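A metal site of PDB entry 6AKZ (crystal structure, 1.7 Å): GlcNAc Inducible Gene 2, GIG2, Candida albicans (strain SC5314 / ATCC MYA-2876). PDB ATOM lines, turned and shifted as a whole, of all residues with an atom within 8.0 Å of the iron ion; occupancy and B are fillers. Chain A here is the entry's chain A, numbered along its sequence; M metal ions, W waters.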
ATOM      1  N   TRP A 127      18.814 -23.075  26.741  1.00  0.00           N
ATOM      2  CA  TRP A 127      18.498 -24.191  25.854  1.00  0.00           C
ATOM      3  C   TRP A 127      19.619 -24.432  24.859  1.00  0.00           C
ATOM      4  O   TRP A 127      20.117 -23.492  24.240  1.00  0.00           O
ATOM      5  CB  TRP A 127      17.179 -23.934  25.117  1.00  0.00           C
ATOM      6  CG  TRP A 127      16.007 -23.756  26.020  1.00  0.00           C
ATOM      7  CD1 TRP A 127      15.546 -22.585  26.549  1.00  0.00           C
ATOM      8  CD2 TRP A 127      15.138 -24.791  26.510  1.00  0.00           C
ATOM      9  NE1 TRP A 127      14.446 -22.820  27.331  1.00  0.00           N
ATOM     10  CE2 TRP A 127      14.169 -24.171  27.330  1.00  0.00           C
ATOM     11  CE3 TRP A 127      15.076 -26.175  26.336  1.00  0.00           C
ATOM     12  CZ2 TRP A 127      13.161 -24.883  27.973  1.00  0.00           C
ATOM     13  CZ3 TRP A 127      14.080 -26.886  26.986  1.00  0.00           C
ATOM     14  CH2 TRP A 127      13.136 -26.233  27.791  1.00  0.00           C
ATOM     15  N   LEU A 189       7.713 -18.342  30.467  1.00  0.00           N
ATOM     16  CA  LEU A 189       6.865 -19.347  29.770  1.00  0.00           C
ATOM     17  C   LEU A 189       5.784 -19.844  30.753  1.00  0.00           C
ATOM     18  O   LEU A 189       6.080 -20.605  31.629  1.00  0.00           O
ATOM     19  CB  LEU A 189       7.719 -20.518  29.289  1.00  0.00           C
ATOM     20  N   PRO A 190       4.537 -19.332  30.662  1.00  0.00           N
ATOM     21  CA  PRO A 190       3.561 -19.598  31.725  1.00  0.00           C
ATOM     22  C   PRO A 190       2.871 -20.979  31.670  1.00  0.00           C
ATOM     23  O   PRO A 190       3.187 -21.771  30.786  1.00  0.00           O
ATOM     24  CB  PRO A 190       2.548 -18.479  31.523  1.00  0.00           C
ATOM     25  CG  PRO A 190       2.519 -18.321  30.073  1.00  0.00           C
ATOM     26  CD  PRO A 190       3.956 -18.476  29.625  1.00  0.00           C
ATOM     27  N   LEU A 191       1.989 -21.260  32.630  1.00  0.00           N
ATOM     28  CA  LEU A 191       1.227 -22.520  32.684  1.00  0.00           C
ATOM     29  C   LEU A 191       0.546 -22.847  31.353  1.00  0.00           C
ATOM     30  O   LEU A 191      -0.177 -22.007  30.782  1.00  0.00           O
ATOM     31  CB  LEU A 191       0.195 -22.565  33.810  1.00  0.00           C
ATOM     32  CG  LEU A 191      -0.412 -23.914  34.097  1.00  0.00           C
ATOM     33  CD1 LEU A 191       0.593 -24.670  34.982  1.00  0.00           C
ATOM     34  CD2 LEU A 191      -1.719 -23.743  34.836  1.00  0.00           C
ATOM     35  N   HIS A 192       0.753 -24.074  30.868  1.00  0.00           N
ATOM     36  CA  HIS A 192       0.222 -24.433  29.600  1.00  0.00           C
ATOM     37  C   HIS A 192       0.072 -25.961  29.445  1.00  0.00           C
ATOM     38  O   HIS A 192       0.671 -26.737  30.205  1.00  0.00           O
ATOM     39  CB  HIS A 192       1.257 -23.909  28.494  1.00  0.00           C
ATOM     40  CG  HIS A 192       2.616 -24.532  28.566  1.00  0.00           C
ATOM     41  ND1 HIS A 192       3.594 -24.124  29.426  1.00  0.00           N
ATOM     42  CD2 HIS A 192       3.141 -25.547  27.856  1.00  0.00           C
ATOM     43  CE1 HIS A 192       4.657 -24.894  29.296  1.00  0.00           C
ATOM     44  NE2 HIS A 192       4.409 -25.735  28.315  1.00  0.00           N
ATOM     45  N   LEU A 193      -0.516 -26.328  28.329  1.00  0.00           N
ATOM     46  CA  LEU A 193      -0.481 -27.645  27.793  1.00  0.00           C
ATOM     47  C   LEU A 193       0.319 -27.569  26.438  1.00  0.00           C
ATOM     48  O   LEU A 193       0.295 -26.617  25.792  1.00  0.00           O
ATOM     49  CB  LEU A 193      -1.833 -28.199  27.460  1.00  0.00           C
ATOM     50  CG  LEU A 193      -2.875 -28.360  28.541  1.00  0.00           C
ATOM     51  CD1 LEU A 193      -4.059 -29.071  27.971  1.00  0.00           C
ATOM     52  CD2 LEU A 193      -2.317 -29.110  29.708  1.00  0.00           C
ATOM     53  N   ASP A 194       1.069 -28.621  26.113  1.00  0.00           N
ATOM     54  CA  ASP A 194       1.738 -28.718  24.842  1.00  0.00           C
ATOM     55  C   ASP A 194       0.779 -29.652  24.011  1.00  0.00           C
ATOM     56  O   ASP A 194      -0.364 -29.761  24.340  1.00  0.00           O
ATOM     57  CB  ASP A 194       3.154 -29.275  24.984  1.00  0.00           C
ATOM     58  CG  ASP A 194       4.062 -28.295  25.661  1.00  0.00           C
ATOM     59  OD1 ASP A 194       4.238 -27.255  25.041  1.00  0.00           O
ATOM     60  OD2 ASP A 194       4.491 -28.582  26.766  1.00  0.00           O
ATOM     61  N   SER A 195       1.270 -30.296  22.973  1.00  0.00           N
ATOM     62  CA  SER A 195       0.462 -31.176  22.181  1.00  0.00           C
ATOM     63  C   SER A 195      -0.787 -30.493  21.571  1.00  0.00           C
ATOM     64  O   SER A 195      -1.820 -31.060  21.466  1.00  0.00           O
ATOM     65  CB  SER A 195       0.093 -32.474  22.908  1.00  0.00           C
ATOM     66  OG  SER A 195       1.241 -33.183  23.296  1.00  0.00           O
ATOM     67  N   ARG A 254       3.488 -37.634  21.441  1.00  0.00           N
ATOM     68  CA  ARG A 254       4.176 -38.146  22.639  1.00  0.00           C
ATOM     69  C   ARG A 254       3.036 -38.379  23.660  1.00  0.00           C
ATOM     70  O   ARG A 254       2.194 -37.483  23.842  1.00  0.00           O
ATOM     71  CB  ARG A 254       5.168 -37.107  23.205  1.00  0.00           C
ATOM     72  CG  ARG A 254       6.295 -36.719  22.230  1.00  0.00           C
ATOM     73  CD  ARG A 254       7.168 -35.625  22.785  1.00  0.00           C
ATOM     74  NE  ARG A 254       6.421 -34.368  22.910  1.00  0.00           N
ATOM     75  CZ  ARG A 254       6.894 -33.250  23.470  1.00  0.00           C
ATOM     76  NH1 ARG A 254       8.140 -33.211  23.882  1.00  0.00           N
ATOM     77  NH2 ARG A 254       6.127 -32.154  23.511  1.00  0.00           N
ATOM     78  N   GLN A 257       5.654 -36.551  28.336  1.00  0.00           N
ATOM     79  CA  GLN A 257       6.879 -35.736  28.242  1.00  0.00           C
ATOM     80  C   GLN A 257       7.749 -36.184  29.410  1.00  0.00           C
ATOM     81  O   GLN A 257       7.281 -36.747  30.399  1.00  0.00           O
ATOM     82  CB  GLN A 257       6.622 -34.262  28.424  1.00  0.00           C
ATOM     83  CG  GLN A 257       5.794 -33.618  27.283  1.00  0.00           C
ATOM     84  CD  GLN A 257       5.768 -32.101  27.356  1.00  0.00           C
ATOM     85  OE1 GLN A 257       6.816 -31.493  27.473  1.00  0.00           O
ATOM     86  NE2 GLN A 257       4.601 -31.475  27.176  1.00  0.00           N
ATOM     87  N   LEU A 272      10.625 -27.699  37.434  1.00  0.00           N
ATOM     88  CA  LEU A 272       9.334 -27.860  36.809  1.00  0.00           C
ATOM     89  C   LEU A 272       8.245 -27.715  37.881  1.00  0.00           C
ATOM     90  O   LEU A 272       8.445 -28.093  39.036  1.00  0.00           O
ATOM     91  CB  LEU A 272       9.285 -29.268  36.195  1.00  0.00           C
ATOM     92  CG  LEU A 272       7.994 -29.699  35.434  1.00  0.00           C
ATOM     93  CD1 LEU A 272       7.805 -28.895  34.186  1.00  0.00           C
ATOM     94  CD2 LEU A 272       8.086 -31.183  35.179  1.00  0.00           C
ATOM     95  N   GLY A 320       1.527 -24.554  19.126  1.00  0.00           N
ATOM     96  CA  GLY A 320       1.596 -25.870  19.794  1.00  0.00           C
ATOM     97  C   GLY A 320       1.183 -25.890  21.233  1.00  0.00           C
ATOM     98  O   GLY A 320       1.171 -26.965  21.824  1.00  0.00           O
ATOM     99  N   GLN A 321       0.911 -24.718  21.803  1.00  0.00           N
ATOM    100  CA  GLN A 321       0.676 -24.586  23.230  1.00  0.00           C
ATOM    101  C   GLN A 321      -0.660 -23.983  23.506  1.00  0.00           C
ATOM    102  O   GLN A 321      -1.067 -23.018  22.868  1.00  0.00           O
ATOM    103  CB  GLN A 321       1.738 -23.719  23.914  1.00  0.00           C
ATOM    104  CG  GLN A 321       3.129 -24.282  24.104  1.00  0.00           C
ATOM    105  CD  GLN A 321       3.908 -24.378  22.837  1.00  0.00           C
ATOM    106  OE1 GLN A 321       4.038 -23.388  22.081  1.00  0.00           O
ATOM    107  NE2 GLN A 321       4.433 -25.565  22.574  1.00  0.00           N
ATOM    108  N   PHE A 323      -2.350 -21.913  26.371  1.00  0.00           N
ATOM    109  CA  PHE A 323      -1.988 -21.143  27.542  1.00  0.00           C
ATOM    110  C   PHE A 323      -3.074 -21.069  28.594  1.00  0.00           C
ATOM    111  O   PHE A 323      -4.242 -20.849  28.320  1.00  0.00           O
ATOM    112  CB  PHE A 323      -1.455 -19.784  27.090  1.00  0.00           C
ATOM    113  CG  PHE A 323      -0.093 -19.891  26.557  1.00  0.00           C
ATOM    114  CD1 PHE A 323       0.934 -20.244  27.409  1.00  0.00           C
ATOM    115  CD2 PHE A 323       0.168 -19.748  25.204  1.00  0.00           C
ATOM    116  CE1 PHE A 323       2.223 -20.384  26.958  1.00  0.00           C
ATOM    117  CE2 PHE A 323       1.454 -19.877  24.744  1.00  0.00           C
ATOM    118  CZ  PHE A 323       2.482 -20.204  25.615  1.00  0.00           C
ATOM    119  N   TRP A 349       5.654 -36.577  32.750  1.00  0.00           N
ATOM    120  CA  TRP A 349       4.337 -36.103  32.906  1.00  0.00           C
ATOM    121  C   TRP A 349       3.500 -36.391  31.640  1.00  0.00           C
ATOM    122  O   TRP A 349       3.951 -36.369  30.477  1.00  0.00           O
ATOM    123  CB  TRP A 349       4.225 -34.643  33.326  1.00  0.00           C
ATOM    124  CG  TRP A 349       4.788 -33.622  32.376  1.00  0.00           C
ATOM    125  CD1 TRP A 349       4.077 -32.833  31.539  1.00  0.00           C
ATOM    126  CD2 TRP A 349       6.178 -33.300  32.151  1.00  0.00           C
ATOM    127  NE1 TRP A 349       4.940 -31.993  30.754  1.00  0.00           N
ATOM    128  CE2 TRP A 349       6.219 -32.224  31.191  1.00  0.00           C
ATOM    129  CE3 TRP A 349       7.380 -33.757  32.710  1.00  0.00           C
ATOM    130  CZ2 TRP A 349       7.421 -31.627  30.803  1.00  0.00           C
ATOM    131  CZ3 TRP A 349       8.598 -33.190  32.256  1.00  0.00           C
ATOM    132  CH2 TRP A 349       8.608 -32.151  31.332  1.00  0.00           C
ATOM    133  N   LEU A 353      -0.974 -32.837  30.999  1.00  0.00           N
ATOM    134  CA  LEU A 353      -0.819 -32.247  32.311  1.00  0.00           C
ATOM    135  C   LEU A 353      -0.356 -30.768  32.232  1.00  0.00           C
ATOM    136  O   LEU A 353       0.631 -30.412  31.518  1.00  0.00           O
ATOM    137  CB  LEU A 353       0.197 -33.038  33.137  1.00  0.00           C
ATOM    138  CG  LEU A 353      -0.042 -32.902  34.606  1.00  0.00           C
ATOM    139  CD1 LEU A 353      -1.290 -33.672  35.007  1.00  0.00           C
ATOM    140  CD2 LEU A 353       1.121 -33.372  35.477  1.00  0.00           C
ATOM    141  N   PRO A 354      -1.119 -29.876  32.851  1.00  0.00           N
ATOM    142  CA  PRO A 354      -0.630 -28.487  32.906  1.00  0.00           C
ATOM    143  C   PRO A 354       0.711 -28.425  33.632  1.00  0.00           C
ATOM    144  O   PRO A 354       0.851 -29.005  34.702  1.00  0.00           O
ATOM    145  CB  PRO A 354      -1.737 -27.792  33.689  1.00  0.00           C
ATOM    146  CG  PRO A 354      -2.930 -28.685  33.652  1.00  0.00           C
ATOM    147  CD  PRO A 354      -2.419 -30.038  33.526  1.00  0.00           C
ATOM    148  N   HIS A 355       1.645 -27.617  33.080  1.00  0.00           N
ATOM    149  CA  HIS A 355       2.928 -27.511  33.674  1.00  0.00           C
ATOM    150  C   HIS A 355       3.535 -26.175  33.267  1.00  0.00           C
ATOM    151  O   HIS A 355       3.042 -25.487  32.336  1.00  0.00           O
ATOM    152  CB  HIS A 355       3.801 -28.676  33.252  1.00  0.00           C
ATOM    153  CG  HIS A 355       4.005 -28.720  31.784  1.00  0.00           C
ATOM    154  ND1 HIS A 355       3.036 -29.168  30.929  1.00  0.00           N
ATOM    155  CD2 HIS A 355       5.026 -28.278  31.000  1.00  0.00           C
ATOM    156  CE1 HIS A 355       3.464 -29.041  29.674  1.00  0.00           C
ATOM    157  NE2 HIS A 355       4.650 -28.503  29.705  1.00  0.00           N
ATOM    158  N   GLU A 356       4.547 -25.786  33.997  1.00  0.00           N
ATOM    159  CA  GLU A 356       5.396 -24.589  33.623  1.00  0.00           C
ATOM    160  C   GLU A 356       6.740 -24.769  34.304  1.00  0.00           C
ATOM    161  O   GLU A 356       6.890 -25.620  35.174  1.00  0.00           O
ATOM    162  CB  GLU A 356       4.755 -23.304  34.157  1.00  0.00           C
ATOM    163  CG  GLU A 356       4.423 -23.344  35.620  1.00  0.00           C
ATOM    164  CD  GLU A 356       3.802 -22.061  36.235  1.00  0.00           C
ATOM    165  OE1 GLU A 356       3.420 -21.143  35.483  1.00  0.00           O
ATOM    166  OE2 GLU A 356       3.717 -22.003  37.500  1.00  0.00           O
ATOM    167  N   VAL A 357       7.727 -23.992  33.889  1.00  0.00           N
ATOM    168  CA  VAL A 357       9.051 -23.980  34.583  1.00  0.00           C
ATOM    169  C   VAL A 357       9.049 -22.898  35.627  1.00  0.00           C
ATOM    170  O   VAL A 357       8.253 -21.955  35.594  1.00  0.00           O
ATOM    171  CB  VAL A 357      10.270 -23.796  33.690  1.00  0.00           C
ATOM    172  CG1 VAL A 357      10.670 -25.150  33.088  1.00  0.00           C
ATOM    173  CG2 VAL A 357      10.033 -22.712  32.678  1.00  0.00           C
ATOM    174  N   TYR A 371      16.031 -33.825  27.815  1.00  0.00           N
ATOM    175  CA  TYR A 371      14.652 -34.089  27.435  1.00  0.00           C
ATOM    176  C   TYR A 371      14.557 -35.378  26.639  1.00  0.00           C
ATOM    177  O   TYR A 371      15.314 -35.566  25.694  1.00  0.00           O
ATOM    178  CB  TYR A 371      14.027 -32.973  26.608  1.00  0.00           C
ATOM    179  CG  TYR A 371      13.781 -31.714  27.493  1.00  0.00           C
ATOM    180  CD1 TYR A 371      12.613 -31.561  28.213  1.00  0.00           C
ATOM    181  CD2 TYR A 371      14.782 -30.773  27.634  1.00  0.00           C
ATOM    182  CE1 TYR A 371      12.413 -30.446  29.054  1.00  0.00           C
ATOM    183  CE2 TYR A 371      14.567 -29.648  28.458  1.00  0.00           C
ATOM    184  CZ  TYR A 371      13.412 -29.497  29.158  1.00  0.00           C
ATOM    185  OH  TYR A 371      13.231 -28.402  30.024  1.00  0.00           O
HETATM  186 FE    FE M   1       5.673 -27.444  28.013  1.00  0.00          FE
HETATM  187  O   HOH W   1       7.322 -26.568  29.143  1.00  0.00           O
HETATM  188  O   HOH W   2       7.154 -28.857  27.687  1.00  0.00           O
HETATM  189  O   HOH W   3       6.603 -26.487  26.257  1.00  0.00           O
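A ring nitrogen (ND1) of His 355 is in hydrogen-bond range of the indole nitrogen (NE1) of Trp 349 (3.4 Å). The side-chain amide nitrogen (NE2) of Gln 257 sits close to the side-chain carboxylate (OD2) of Asp 194 (2.9 Å). A ring nitrogen (ND1) of His 192 lies within hydrogen-bond range of the backbone carbonyl oxygen of Pro 190. ND1 of His 355 lies within hydrogen-bond range of O of Leu 353 (2.8 Å). OD1 of Asp 194 is in hydrogen-bond range of NE2 of Gln 321 (3.0 Å).
Of the 21 residues printed, 3 come within 4 Å of the iron ion.
The iron ion is bound by the side-chain carboxylate (OD2) of Asp 194 (2.1 Å), water W2 (2.1 Å), a ring nitrogen (NE2) of His 192 (2.1 Å), water W1 (2.2 Å), water W3 (2.2 Å) and a ring nitrogen (NE2) of His 355 (2.2 Å). The iron ion has six donor atoms within binding distance.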
